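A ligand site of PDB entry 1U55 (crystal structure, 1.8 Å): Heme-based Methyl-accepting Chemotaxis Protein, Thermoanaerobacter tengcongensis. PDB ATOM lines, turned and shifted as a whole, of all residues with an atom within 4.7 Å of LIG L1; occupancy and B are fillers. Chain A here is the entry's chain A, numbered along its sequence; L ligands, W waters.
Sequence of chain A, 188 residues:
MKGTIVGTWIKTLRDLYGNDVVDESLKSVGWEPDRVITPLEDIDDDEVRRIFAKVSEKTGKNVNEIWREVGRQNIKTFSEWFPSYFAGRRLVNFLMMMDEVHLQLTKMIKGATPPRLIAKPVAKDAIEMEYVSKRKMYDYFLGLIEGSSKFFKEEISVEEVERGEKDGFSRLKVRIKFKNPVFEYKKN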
ATOM      1  N   MET A   1      -1.549 -20.578   1.709  1.00  0.00           N
ATOM      2  CA  MET A   1      -0.562 -19.657   2.347  1.00  0.00           C
ATOM      3  C   MET A   1      -0.272 -20.170   3.754  1.00  0.00           C
ATOM      4  O   MET A   1      -1.209 -20.497   4.500  1.00  0.00           O
ATOM      5  CB  MET A   1      -1.140 -18.239   2.434  1.00  0.00           C
ATOM      6  CG  MET A   1      -0.099 -17.160   2.636  1.00  0.00           C
ATOM      7  SD  MET A   1       0.899 -16.949   1.150  1.00  0.00           S
ATOM      8  CE  MET A   1      -0.294 -16.168   0.074  1.00  0.00           C
ATOM      9  N   LYS A   2       0.999 -20.245   4.122  1.00  0.00           N
ATOM     10  CA  LYS A   2       1.362 -20.742   5.445  1.00  0.00           C
ATOM     11  C   LYS A   2       0.546 -20.003   6.508  1.00  0.00           C
ATOM     12  O   LYS A   2       0.519 -18.771   6.544  1.00  0.00           O
ATOM     13  CB  LYS A   2       2.855 -20.545   5.693  1.00  0.00           C
ATOM     14  CG  LYS A   2       3.328 -21.044   7.052  1.00  0.00           C
ATOM     15  CD  LYS A   2       4.847 -21.039   7.155  1.00  0.00           C
ATOM     16  CE  LYS A   2       5.332 -21.276   8.579  1.00  0.00           C
ATOM     17  NZ  LYS A   2       4.792 -22.529   9.179  1.00  0.00           N
ATOM     18  N   ILE A   5       1.930 -17.127   8.770  1.00  0.00           N
ATOM     19  CA  ILE A   5       2.186 -15.902   8.016  1.00  0.00           C
ATOM     20  C   ILE A   5       0.872 -15.143   7.886  1.00  0.00           C
ATOM     21  O   ILE A   5       0.835 -13.910   8.009  1.00  0.00           O
ATOM     22  CB  ILE A   5       2.770 -16.212   6.629  1.00  0.00           C
ATOM     23  CG1 ILE A   5       4.017 -17.092   6.779  1.00  0.00           C
ATOM     24  CG2 ILE A   5       3.099 -14.915   5.905  1.00  0.00           C
ATOM     25  CD1 ILE A   5       5.111 -16.475   7.666  1.00  0.00           C
ATOM     26  N   TRP A   9      -0.346 -11.176   9.054  1.00  0.00           N
ATOM     27  CA  TRP A   9      -1.160 -10.229   8.305  1.00  0.00           C
ATOM     28  C   TRP A   9      -2.370  -9.784   9.115  1.00  0.00           C
ATOM     29  O   TRP A   9      -2.757  -8.621   9.061  1.00  0.00           O
ATOM     30  CB  TRP A   9      -1.621 -10.821   6.966  1.00  0.00           C
ATOM     31  CG  TRP A   9      -0.470 -11.142   6.052  1.00  0.00           C
ATOM     32  CD1 TRP A   9       0.804 -10.642   6.123  1.00  0.00           C
ATOM     33  CD2 TRP A   9      -0.486 -12.050   4.951  1.00  0.00           C
ATOM     34  NE1 TRP A   9       1.586 -11.188   5.128  1.00  0.00           N
ATOM     35  CE2 TRP A   9       0.819 -12.056   4.391  1.00  0.00           C
ATOM     36  CE3 TRP A   9      -1.473 -12.861   4.364  1.00  0.00           C
ATOM     37  CZ2 TRP A   9       1.152 -12.840   3.281  1.00  0.00           C
ATOM     38  CZ3 TRP A   9      -1.132 -13.630   3.264  1.00  0.00           C
ATOM     39  CH2 TRP A   9       0.171 -13.616   2.735  1.00  0.00           C
ATOM     40  N   ILE A  75       6.856  -5.940   8.313  1.00  0.00           N
ATOM     41  CA  ILE A  75       8.235  -6.232   8.714  1.00  0.00           C
ATOM     42  C   ILE A  75       8.344  -6.066  10.234  1.00  0.00           C
ATOM     43  O   ILE A  75       9.021  -6.845  10.892  1.00  0.00           O
ATOM     44  CB  ILE A  75       9.246  -5.308   8.004  1.00  0.00           C
ATOM     45  CG1 ILE A  75       9.270  -5.632   6.502  1.00  0.00           C
ATOM     46  CG2 ILE A  75      10.652  -5.502   8.614  1.00  0.00           C
ATOM     47  CD1 ILE A  75       9.826  -7.031   6.179  1.00  0.00           C
ATOM     48  N   PHE A  78       6.893  -9.150  11.711  1.00  0.00           N
ATOM     49  CA  PHE A  78       7.856 -10.245  11.576  1.00  0.00           C
ATOM     50  C   PHE A  78       8.989 -10.124  12.603  1.00  0.00           C
ATOM     51  O   PHE A  78       9.437 -11.122  13.182  1.00  0.00           O
ATOM     52  CB  PHE A  78       8.483 -10.245  10.173  1.00  0.00           C
ATOM     53  CG  PHE A  78       7.665 -10.954   9.125  1.00  0.00           C
ATOM     54  CD1 PHE A  78       7.565 -10.428   7.830  1.00  0.00           C
ATOM     55  CD2 PHE A  78       7.042 -12.171   9.391  1.00  0.00           C
ATOM     56  CE1 PHE A  78       6.858 -11.108   6.829  1.00  0.00           C
ATOM     57  CE2 PHE A  78       6.335 -12.851   8.391  1.00  0.00           C
ATOM     58  CZ  PHE A  78       6.246 -12.316   7.113  1.00  0.00           C
ATOM     59  N   PHE A  82       9.179 -13.349  14.640  1.00  0.00           N
ATOM     60  CA  PHE A  82      10.289 -14.158  14.139  1.00  0.00           C
ATOM     61  C   PHE A  82      11.592 -13.385  14.305  1.00  0.00           C
ATOM     62  O   PHE A  82      12.330 -13.189  13.337  1.00  0.00           O
ATOM     63  CB  PHE A  82      10.079 -14.505  12.658  1.00  0.00           C
ATOM     64  CG  PHE A  82       8.812 -15.253  12.361  1.00  0.00           C
ATOM     65  CD1 PHE A  82       7.594 -14.592  12.288  1.00  0.00           C
ATOM     66  CD2 PHE A  82       8.843 -16.630  12.146  1.00  0.00           C
ATOM     67  CE1 PHE A  82       6.414 -15.293  12.010  1.00  0.00           C
ATOM     68  CE2 PHE A  82       7.671 -17.347  11.865  1.00  0.00           C
ATOM     69  CZ  PHE A  82       6.453 -16.672  11.789  1.00  0.00           C
ATOM     70  N   TYR A  85      15.377 -14.045  12.643  1.00  0.00           N
ATOM     71  CA  TYR A  85      15.719 -13.710  11.268  1.00  0.00           C
ATOM     72  C   TYR A  85      16.234 -12.278  11.117  1.00  0.00           C
ATOM     73  O   TYR A  85      16.638 -11.884  10.027  1.00  0.00           O
ATOM     74  CB  TYR A  85      14.496 -13.892  10.350  1.00  0.00           C
ATOM     75  CG  TYR A  85      14.040 -15.325  10.230  1.00  0.00           C
ATOM     76  CD1 TYR A  85      13.048 -15.831  11.079  1.00  0.00           C
ATOM     77  CD2 TYR A  85      14.608 -16.175   9.297  1.00  0.00           C
ATOM     78  CE1 TYR A  85      12.654 -17.168  11.001  1.00  0.00           C
ATOM     79  CE2 TYR A  85      14.232 -17.514   9.210  1.00  0.00           C
ATOM     80  CZ  TYR A  85      13.249 -17.991  10.067  1.00  0.00           C
ATOM     81  OH  TYR A  85      12.892 -19.323   9.992  1.00  0.00           O
ATOM     82  N   PHE A  86      16.204 -11.515  12.198  1.00  0.00           N
ATOM     83  CA  PHE A  86      16.652 -10.125  12.148  1.00  0.00           C
ATOM     84  C   PHE A  86      17.945  -9.873  12.920  1.00  0.00           C
ATOM     85  O   PHE A  86      18.772  -9.061  12.517  1.00  0.00           O
ATOM     86  CB  PHE A  86      15.552  -9.211  12.678  1.00  0.00           C
ATOM     87  CG  PHE A  86      14.322  -9.189  11.811  1.00  0.00           C
ATOM     88  CD1 PHE A  86      14.116  -8.174  10.888  1.00  0.00           C
ATOM     89  CD2 PHE A  86      13.384 -10.211  11.904  1.00  0.00           C
ATOM     90  CE1 PHE A  86      12.992  -8.176  10.054  1.00  0.00           C
ATOM     91  CE2 PHE A  86      12.262 -10.234  11.079  1.00  0.00           C
ATOM     92  CZ  PHE A  86      12.065  -9.206  10.149  1.00  0.00           C
ATOM     93  N   PHE A  94      19.957  -9.728   5.000  1.00  0.00           N
ATOM     94  CA  PHE A  94      18.557 -10.079   5.243  1.00  0.00           C
ATOM     95  C   PHE A  94      17.887 -10.410   3.907  1.00  0.00           C
ATOM     96  O   PHE A  94      17.316 -11.482   3.740  1.00  0.00           O
ATOM     97  CB  PHE A  94      17.852  -8.898   5.908  1.00  0.00           C
ATOM     98  CG  PHE A  94      16.393  -9.148   6.204  1.00  0.00           C
ATOM     99  CD1 PHE A  94      16.008  -9.993   7.235  1.00  0.00           C
ATOM    100  CD2 PHE A  94      15.402  -8.512   5.457  1.00  0.00           C
ATOM    101  CE1 PHE A  94      14.655 -10.216   7.525  1.00  0.00           C
ATOM    102  CE2 PHE A  94      14.046  -8.716   5.737  1.00  0.00           C
ATOM    103  CZ  PHE A  94      13.673  -9.568   6.771  1.00  0.00           C
ATOM    104  N   LEU A  95      17.978  -9.484   2.966  1.00  0.00           N
ATOM    105  CA  LEU A  95      17.370  -9.685   1.660  1.00  0.00           C
ATOM    106  C   LEU A  95      17.902 -10.912   0.903  1.00  0.00           C
ATOM    107  O   LEU A  95      17.125 -11.652   0.319  1.00  0.00           O
ATOM    108  CB  LEU A  95      17.537  -8.422   0.796  1.00  0.00           C
ATOM    109  CG  LEU A  95      16.757  -7.196   1.310  1.00  0.00           C
ATOM    110  CD1 LEU A  95      17.080  -5.993   0.455  1.00  0.00           C
ATOM    111  CD2 LEU A  95      15.265  -7.499   1.287  1.00  0.00           C
ATOM    112  N   MET A  98      16.339 -14.333   2.005  1.00  0.00           N
ATOM    113  CA  MET A  98      14.900 -14.563   1.886  1.00  0.00           C
ATOM    114  C   MET A  98      14.483 -15.752   1.025  1.00  0.00           C
ATOM    115  O   MET A  98      13.584 -16.498   1.402  1.00  0.00           O
ATOM    116  CB  MET A  98      14.198 -13.294   1.392  1.00  0.00           C
ATOM    117  CG  MET A  98      14.134 -12.176   2.428  1.00  0.00           C
ATOM    118  SD  MET A  98      13.273 -12.662   3.954  1.00  0.00           S
ATOM    119  CE  MET A  98      14.639 -12.950   5.090  1.00  0.00           C
ATOM    120  N   VAL A 101      14.796 -18.798   3.107  1.00  0.00           N
ATOM    121  CA  VAL A 101      13.861 -18.790   4.218  1.00  0.00           C
ATOM    122  C   VAL A 101      12.481 -19.225   3.765  1.00  0.00           C
ATOM    123  O   VAL A 101      11.807 -20.002   4.436  1.00  0.00           O
ATOM    124  CB  VAL A 101      13.758 -17.391   4.864  1.00  0.00           C
ATOM    125  CG1 VAL A 101      12.547 -17.315   5.787  1.00  0.00           C
ATOM    126  CG2 VAL A 101      15.029 -17.096   5.667  1.00  0.00           C
ATOM    127  N   HIS A 102      12.042 -18.738   2.601  1.00  0.00           N
ATOM    128  CA  HIS A 102      10.732 -19.107   2.107  1.00  0.00           C
ATOM    129  C   HIS A 102      10.658 -20.586   1.711  1.00  0.00           C
ATOM    130  O   HIS A 102       9.617 -21.211   1.851  1.00  0.00           O
ATOM    131  CB  HIS A 102      10.307 -18.186   0.961  1.00  0.00           C
ATOM    132  CG  HIS A 102       9.964 -16.807   1.427  1.00  0.00           C
ATOM    133  ND1 HIS A 102      10.897 -15.949   1.965  1.00  0.00           N
ATOM    134  CD2 HIS A 102       8.776 -16.163   1.519  1.00  0.00           C
ATOM    135  CE1 HIS A 102      10.303 -14.843   2.371  1.00  0.00           C
ATOM    136  NE2 HIS A 102       9.009 -14.947   2.121  1.00  0.00           N
ATOM    137  N   LEU A 105      10.448 -22.523   5.256  1.00  0.00           N
ATOM    138  CA  LEU A 105       9.174 -22.424   5.950  1.00  0.00           C
ATOM    139  C   LEU A 105       7.976 -23.061   5.240  1.00  0.00           C
ATOM    140  O   LEU A 105       6.894 -23.155   5.817  1.00  0.00           O
ATOM    141  CB  LEU A 105       8.873 -20.950   6.274  1.00  0.00           C
ATOM    142  CG  LEU A 105       9.914 -20.225   7.135  1.00  0.00           C
ATOM    143  CD1 LEU A 105       9.393 -18.866   7.533  1.00  0.00           C
ATOM    144  CD2 LEU A 105      10.232 -21.044   8.370  1.00  0.00           C
ATOM    145  N   THR A 106       8.158 -23.504   3.999  1.00  0.00           N
ATOM    146  CA  THR A 106       7.059 -24.132   3.256  1.00  0.00           C
ATOM    147  C   THR A 106       7.350 -25.584   2.886  1.00  0.00           C
ATOM    148  O   THR A 106       6.485 -26.259   2.311  1.00  0.00           O
ATOM    149  CB  THR A 106       6.717 -23.374   1.953  1.00  0.00           C
ATOM    150  OG1 THR A 106       7.874 -23.281   1.112  1.00  0.00           O
ATOM    151  CG2 THR A 106       6.191 -21.972   2.266  1.00  0.00           C
ATOM    152  N   THR A 113       4.106 -23.881  -2.800  1.00  0.00           N
ATOM    153  CA  THR A 113       4.341 -22.923  -3.867  1.00  0.00           C
ATOM    154  C   THR A 113       4.790 -21.584  -3.289  1.00  0.00           C
ATOM    155  O   THR A 113       4.110 -20.576  -3.410  1.00  0.00           O
ATOM    156  CB  THR A 113       3.059 -22.702  -4.723  1.00  0.00           C
ATOM    157  OG1 THR A 113       2.033 -22.119  -3.913  1.00  0.00           O
ATOM    158  CG2 THR A 113       2.567 -24.034  -5.278  1.00  0.00           C
ATOM    159  N   PRO A 114       5.962 -21.578  -2.621  1.00  0.00           N
ATOM    160  CA  PRO A 114       6.436 -20.322  -2.055  1.00  0.00           C
ATOM    161  C   PRO A 114       6.931 -19.412  -3.158  1.00  0.00           C
ATOM    162  O   PRO A 114       7.261 -19.855  -4.253  1.00  0.00           O
ATOM    163  CB  PRO A 114       7.572 -20.761  -1.146  1.00  0.00           C
ATOM    164  CG  PRO A 114       8.161 -21.911  -1.928  1.00  0.00           C
ATOM    165  CD  PRO A 114       6.916 -22.668  -2.351  1.00  0.00           C
ATOM    166  N   PRO A 115       6.977 -18.109  -2.886  1.00  0.00           N
ATOM    167  CA  PRO A 115       7.471 -17.199  -3.906  1.00  0.00           C
ATOM    168  C   PRO A 115       8.991 -17.351  -3.964  1.00  0.00           C
ATOM    169  O   PRO A 115       9.635 -17.611  -2.937  1.00  0.00           O
ATOM    170  CB  PRO A 115       7.059 -15.826  -3.376  1.00  0.00           C
ATOM    171  CG  PRO A 115       7.168 -16.008  -1.875  1.00  0.00           C
ATOM    172  CD  PRO A 115       6.535 -17.381  -1.682  1.00  0.00           C
ATOM    173  N   LEU A 117      12.557 -15.565  -4.460  1.00  0.00           N
ATOM    174  CA  LEU A 117      13.035 -14.196  -4.238  1.00  0.00           C
ATOM    175  C   LEU A 117      14.539 -14.088  -4.427  1.00  0.00           C
ATOM    176  O   LEU A 117      15.233 -13.425  -3.655  1.00  0.00           O
ATOM    177  CB  LEU A 117      12.678 -13.786  -2.804  1.00  0.00           C
ATOM    178  CG  LEU A 117      11.189 -13.931  -2.447  1.00  0.00           C
ATOM    179  CD1 LEU A 117      11.024 -13.894  -0.926  1.00  0.00           C
ATOM    180  CD2 LEU A 117      10.387 -12.804  -3.104  1.00  0.00           C
ATOM    181  N   MET A 129      16.804  -8.197  -7.261  1.00  0.00           N
ATOM    182  CA  MET A 129      15.973  -9.198  -6.619  1.00  0.00           C
ATOM    183  C   MET A 129      14.803  -9.470  -7.539  1.00  0.00           C
ATOM    184  O   MET A 129      14.116  -8.550  -7.964  1.00  0.00           O
ATOM    185  CB  MET A 129      15.474  -8.690  -5.264  1.00  0.00           C
ATOM    186  CG  MET A 129      14.751  -9.755  -4.445  1.00  0.00           C
ATOM    187  SD  MET A 129      14.374  -9.185  -2.759  1.00  0.00           S
ATOM    188  CE  MET A 129      15.982  -9.105  -2.095  1.00  0.00           C
ATOM    189  N   TYR A 131      11.224 -11.329  -7.975  1.00  0.00           N
ATOM    190  CA  TYR A 131      10.066 -11.973  -7.366  1.00  0.00           C
ATOM    191  C   TYR A 131       9.444 -12.853  -8.445  1.00  0.00           C
ATOM    192  O   TYR A 131       9.216 -12.393  -9.553  1.00  0.00           O
ATOM    193  CB  TYR A 131       9.055 -10.899  -6.955  1.00  0.00           C
ATOM    194  CG  TYR A 131       7.669 -11.440  -6.647  1.00  0.00           C
ATOM    195  CD1 TYR A 131       7.399 -12.091  -5.443  1.00  0.00           C
ATOM    196  CD2 TYR A 131       6.633 -11.314  -7.572  1.00  0.00           C
ATOM    197  CE1 TYR A 131       6.121 -12.595  -5.160  1.00  0.00           C
ATOM    198  CE2 TYR A 131       5.343 -11.810  -7.291  1.00  0.00           C
ATOM    199  CZ  TYR A 131       5.105 -12.446  -6.076  1.00  0.00           C
ATOM    200  OH  TYR A 131       3.844 -12.936  -5.787  1.00  0.00           O
ATOM    201  N   SER A 133       6.243 -15.702  -8.705  1.00  0.00           N
ATOM    202  CA  SER A 133       5.124 -16.409  -8.069  1.00  0.00           C
ATOM    203  C   SER A 133       3.849 -16.312  -8.895  1.00  0.00           C
ATOM    204  O   SER A 133       3.601 -15.316  -9.571  1.00  0.00           O
ATOM    205  CB  SER A 133       4.850 -15.799  -6.691  1.00  0.00           C
ATOM    206  OG  SER A 133       3.723 -16.409  -6.079  1.00  0.00           O
ATOM    207  N   ARG A 135       1.093 -16.028  -7.597  1.00  0.00           N
ATOM    208  CA  ARG A 135       0.211 -15.146  -6.826  1.00  0.00           C
ATOM    209  C   ARG A 135       0.218 -13.669  -7.226  1.00  0.00           C
ATOM    210  O   ARG A 135      -0.705 -12.930  -6.888  1.00  0.00           O
ATOM    211  CB  ARG A 135       0.529 -15.288  -5.335  1.00  0.00           C
ATOM    212  CG  ARG A 135       0.407 -16.713  -4.803  1.00  0.00           C
ATOM    213  CD  ARG A 135       0.173 -16.712  -3.312  1.00  0.00           C
ATOM    214  NE  ARG A 135       0.024 -18.037  -2.712  1.00  0.00           N
ATOM    215  CZ  ARG A 135       1.029 -18.742  -2.194  1.00  0.00           C
ATOM    216  NH1 ARG A 135       2.258 -18.259  -2.201  1.00  0.00           N
ATOM    217  NH2 ARG A 135       0.780 -19.912  -1.614  1.00  0.00           N
ATOM    218  N   MET A 137       1.787 -10.972  -6.175  1.00  0.00           N
ATOM    219  CA  MET A 137       1.613 -10.063  -5.065  1.00  0.00           C
ATOM    220  C   MET A 137       2.708  -8.992  -5.097  1.00  0.00           C
ATOM    221  O   MET A 137       3.498  -8.860  -4.155  1.00  0.00           O
ATOM    222  CB  MET A 137       1.620 -10.846  -3.756  1.00  0.00           C
ATOM    223  CG  MET A 137       0.366 -11.745  -3.624  1.00  0.00           C
ATOM    224  SD  MET A 137       0.320 -12.884  -2.239  1.00  0.00           S
ATOM    225  CE  MET A 137       0.287 -11.728  -0.840  1.00  0.00           C
ATOM    226  N   TYR A 140       2.695  -6.261  -2.186  1.00  0.00           N
ATOM    227  CA  TYR A 140       3.159  -6.773  -0.903  1.00  0.00           C
ATOM    228  C   TYR A 140       4.682  -6.897  -0.924  1.00  0.00           C
ATOM    229  O   TYR A 140       5.354  -6.498   0.016  1.00  0.00           O
ATOM    230  CB  TYR A 140       2.521  -8.137  -0.618  1.00  0.00           C
ATOM    231  CG  TYR A 140       2.903  -8.736   0.708  1.00  0.00           C
ATOM    232  CD1 TYR A 140       2.685  -8.045   1.912  1.00  0.00           C
ATOM    233  CD2 TYR A 140       3.475 -10.004   0.776  1.00  0.00           C
ATOM    234  CE1 TYR A 140       3.027  -8.609   3.133  1.00  0.00           C
ATOM    235  CE2 TYR A 140       3.820 -10.574   2.005  1.00  0.00           C
ATOM    236  CZ  TYR A 140       3.583  -9.875   3.170  1.00  0.00           C
ATOM    237  OH  TYR A 140       3.969 -10.418   4.362  1.00  0.00           O
ATOM    238  N   PHE A 141       5.189  -7.460  -2.015  1.00  0.00           N
ATOM    239  CA  PHE A 141       6.629  -7.620  -2.239  1.00  0.00           C
ATOM    240  C   PHE A 141       7.345  -6.266  -2.084  1.00  0.00           C
ATOM    241  O   PHE A 141       8.279  -6.136  -1.298  1.00  0.00           O
ATOM    242  CB  PHE A 141       6.851  -8.187  -3.642  1.00  0.00           C
ATOM    243  CG  PHE A 141       8.294  -8.172  -4.103  1.00  0.00           C
ATOM    244  CD1 PHE A 141       9.210  -9.079  -3.581  1.00  0.00           C
ATOM    245  CD2 PHE A 141       8.698  -7.303  -5.108  1.00  0.00           C
ATOM    246  CE1 PHE A 141      10.542  -9.110  -4.063  1.00  0.00           C
ATOM    247  CE2 PHE A 141      10.019  -7.327  -5.592  1.00  0.00           C
ATOM    248  CZ  PHE A 141      10.930  -8.224  -5.060  1.00  0.00           C
ATOM    249  N   LEU A 144       7.205  -4.875   1.513  1.00  0.00           N
ATOM    250  CA  LEU A 144       8.132  -5.515   2.461  1.00  0.00           C
ATOM    251  C   LEU A 144       9.531  -4.939   2.271  1.00  0.00           C
ATOM    252  O   LEU A 144      10.245  -4.719   3.237  1.00  0.00           O
ATOM    253  CB  LEU A 144       8.146  -7.033   2.257  1.00  0.00           C
ATOM    254  CG  LEU A 144       6.857  -7.741   2.688  1.00  0.00           C
ATOM    255  CD1 LEU A 144       6.817  -9.141   2.098  1.00  0.00           C
ATOM    256  CD2 LEU A 144       6.772  -7.789   4.215  1.00  0.00           C
ATOM    257  N   ILE A 145       9.915  -4.707   1.025  1.00  0.00           N
ATOM    258  CA  ILE A 145      11.249  -4.160   0.770  1.00  0.00           C
ATOM    259  C   ILE A 145      11.374  -2.774   1.395  1.00  0.00           C
ATOM    260  O   ILE A 145      12.376  -2.458   2.037  1.00  0.00           O
ATOM    261  CB  ILE A 145      11.539  -4.096  -0.745  1.00  0.00           C
ATOM    262  CG1 ILE A 145      11.639  -5.509  -1.306  1.00  0.00           C
ATOM    263  CG2 ILE A 145      12.863  -3.353  -0.995  1.00  0.00           C
ATOM    264  CD1 ILE A 145      11.800  -5.567  -2.830  1.00  0.00           C
ATOM    265  N   SER A 148      11.553  -3.095   5.049  1.00  0.00           N
ATOM    266  CA  SER A 148      12.841  -3.651   5.470  1.00  0.00           C
ATOM    267  C   SER A 148      13.854  -2.512   5.541  1.00  0.00           C
ATOM    268  O   SER A 148      14.671  -2.467   6.454  1.00  0.00           O
ATOM    269  CB  SER A 148      13.321  -4.719   4.485  1.00  0.00           C
ATOM    270  OG  SER A 148      12.535  -5.905   4.570  1.00  0.00           O
HETATM  271  C1  LIG L   1       4.942 -14.965   1.765  1.00  0.00           C
HETATM  272  C2  LIG L   1       7.943 -15.868   5.472  1.00  0.00           C
HETATM  273  C3  LIG L   1      10.122 -11.658   4.582  1.00  0.00           C
HETATM  274  C4  LIG L   1       8.137 -11.716   0.160  1.00  0.00           C
HETATM  275  C5  LIG L   1       5.590 -15.617   2.815  1.00  0.00           C
HETATM  276  C6  LIG L   1       5.325 -16.989   3.258  1.00  0.00           C
HETATM  277  C7  LIG L   1       6.291 -17.261   4.184  1.00  0.00           C
HETATM  278  C8  LIG L   1       7.035 -16.061   4.417  1.00  0.00           C
HETATM  279  C9  LIG L   1       6.554 -18.619   4.809  1.00  0.00           C
HETATM  280  C10 LIG L   1       4.198 -17.968   2.846  1.00  0.00           C
HETATM  281  C11 LIG L   1       4.459 -18.550   1.456  1.00  0.00           C
HETATM  282  C12 LIG L   1       3.534 -19.699   1.066  1.00  0.00           C
HETATM  283  O1  LIG L   1       3.602 -20.106  -0.098  1.00  0.00           O
HETATM  284  O2  LIG L   1       2.756 -20.192   1.923  1.00  0.00           O
HETATM  285  C13 LIG L   1       8.710 -14.713   5.615  1.00  0.00           C
HETATM  286  C14 LIG L   1       9.526 -14.418   6.767  1.00  0.00           C
HETATM  287  C15 LIG L   1      10.023 -13.154   6.591  1.00  0.00           C
HETATM  288  C16 LIG L   1       9.577 -12.727   5.283  1.00  0.00           C
HETATM  289  C17 LIG L   1       9.615 -15.285   7.998  1.00  0.00           C
HETATM  290  C18 LIG L   1      10.759 -12.324   7.473  1.00  0.00           C
HETATM  291  C19 LIG L   1      11.655 -12.742   8.524  1.00  0.00           C
HETATM  292  C20 LIG L   1       9.846 -11.350   3.242  1.00  0.00           C
HETATM  293  C21 LIG L   1      10.523 -10.336   2.440  1.00  0.00           C
HETATM  294  C22 LIG L   1      10.044 -10.402   1.182  1.00  0.00           C
HETATM  295  C23 LIG L   1       9.040 -11.466   1.211  1.00  0.00           C
HETATM  296  C24 LIG L   1      11.585  -9.371   2.948  1.00  0.00           C
HETATM  297  C25 LIG L   1      10.355  -9.660   0.026  1.00  0.00           C
HETATM  298  C26 LIG L   1      11.531  -8.824  -0.210  1.00  0.00           C
HETATM  299  C27 LIG L   1       6.991 -12.481   0.280  1.00  0.00           C
HETATM  300  C28 LIG L   1       5.861 -12.436  -0.623  1.00  0.00           C
HETATM  301  C29 LIG L   1       4.958 -13.351  -0.180  1.00  0.00           C
HETATM  302  C30 LIG L   1       5.532 -13.937   1.010  1.00  0.00           C
HETATM  303  C31 LIG L   1       5.709 -11.491  -1.804  1.00  0.00           C
HETATM  304  C32 LIG L   1       3.537 -13.591  -0.684  1.00  0.00           C
HETATM  305  C33 LIG L   1       3.186 -14.901  -1.387  1.00  0.00           C
HETATM  306  C34 LIG L   1       3.555 -14.902  -2.864  1.00  0.00           C
HETATM  307  O3  LIG L   1       3.865 -13.824  -3.409  1.00  0.00           O
HETATM  308  O4  LIG L   1       3.528 -15.992  -3.485  1.00  0.00           O
HETATM  309  N1  LIG L   1       6.633 -15.066   3.543  1.00  0.00           N
HETATM  310  N2  LIG L   1       8.730 -13.661   4.715  1.00  0.00           N
HETATM  311  N3  LIG L   1       8.954 -12.044   2.455  1.00  0.00           N
HETATM  312  N4  LIG L   1       6.770 -13.384   1.292  1.00  0.00           N
HETATM  313 FE1  LIG L   1       7.734 -13.499   3.009  1.00  0.00          FE
HETATM  314  O1  LG2 L   2       6.658 -12.244   3.817  1.00  0.00           O
HETATM  315  O2  LG2 L   2       5.417 -12.627   3.982  1.00  0.00           O
HETATM  316  O   HOH W   1       1.409 -22.531   1.125  1.00  0.00           O
HETATM  317  O   HOH W   2       3.444 -22.753  -0.459  1.00  0.00           O
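O of Thr 113 lies close to O1 of LIG L1 (3.4 Å). Residues that only touch LIG L1: Leu 144, Met 98, Met 1, Pro 114, Ile 5, Ile 145, Phe 78, Pro 115, Tyr 85, Leu 105, Met 137, Phe 86, Tyr 140, Thr 106, Leu 117, Phe 94, Phe 141, Met 129 and Ser 148. Along chain A the residues within 4 Å of LIG L1 span positions 1 to 148.
An iron atom (FE1) of LIG L1 is bound by an oxygen (O1) of LG2 L2 (1.8 Å).
The side-chain hydroxyl (OG1) of Thr 106 sits at hydrogen-bond distance from the backbone carbonyl oxygen (O) of His 102. The backbone NH (N) of Met 137 lies within hydrogen-bond range of the side-chain hydroxyl (OH) of Tyr 131, 2.9 Å away. O of Leu 144 is in hydrogen-bond range of OG of Ser 148 (2.9 Å). OH of Tyr 140 lies within hydrogen-bond range of NE1 of Trp 9, at 2.6 Å. A ring nitrogen (ND1) of His 102 is in hydrogen-bond range of the backbone carbonyl oxygen of Met 98 (2.8 Å). The backbone carbonyl oxygen (O) of Thr 113 is in hydrogen-bond range of the guanidinium group (NH1) of Arg 135. The side-chain hydroxyl (OG) of Ser 133 sits close to the side-chain hydroxyl (OH) of Tyr 131. OG of Ser 133 sits close to N of Arg 135 (3.1 Å).
Water W2 bridges an oxygen (O1) of LIG L1 (2.7 Å) and the backbone NH of Thr 113 (2.7 Å).
The side-chain hydroxyl (OH) of Tyr 140 sits at hydrogen-bond distance from an oxygen (O2) of LG2 L2 (2.7 Å). NE2 of His 102 is bound to FE1 of LIG L1, 2.1 Å away. An oxygen (O2) of LIG L1 sits at hydrogen-bond distance from the backbone NH (N) of Lys 2, 2.8 Å away. OH of Tyr 131 lies within hydrogen-bond range of O3 of LIG L1 (2.5 Å). An oxygen (O4) of LIG L1 is in hydrogen-bond range of the side-chain hydroxyl of Ser 133 (2.6 Å). NH1 of Arg 135 is in salt-bridge range of O4 of LIG L1.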
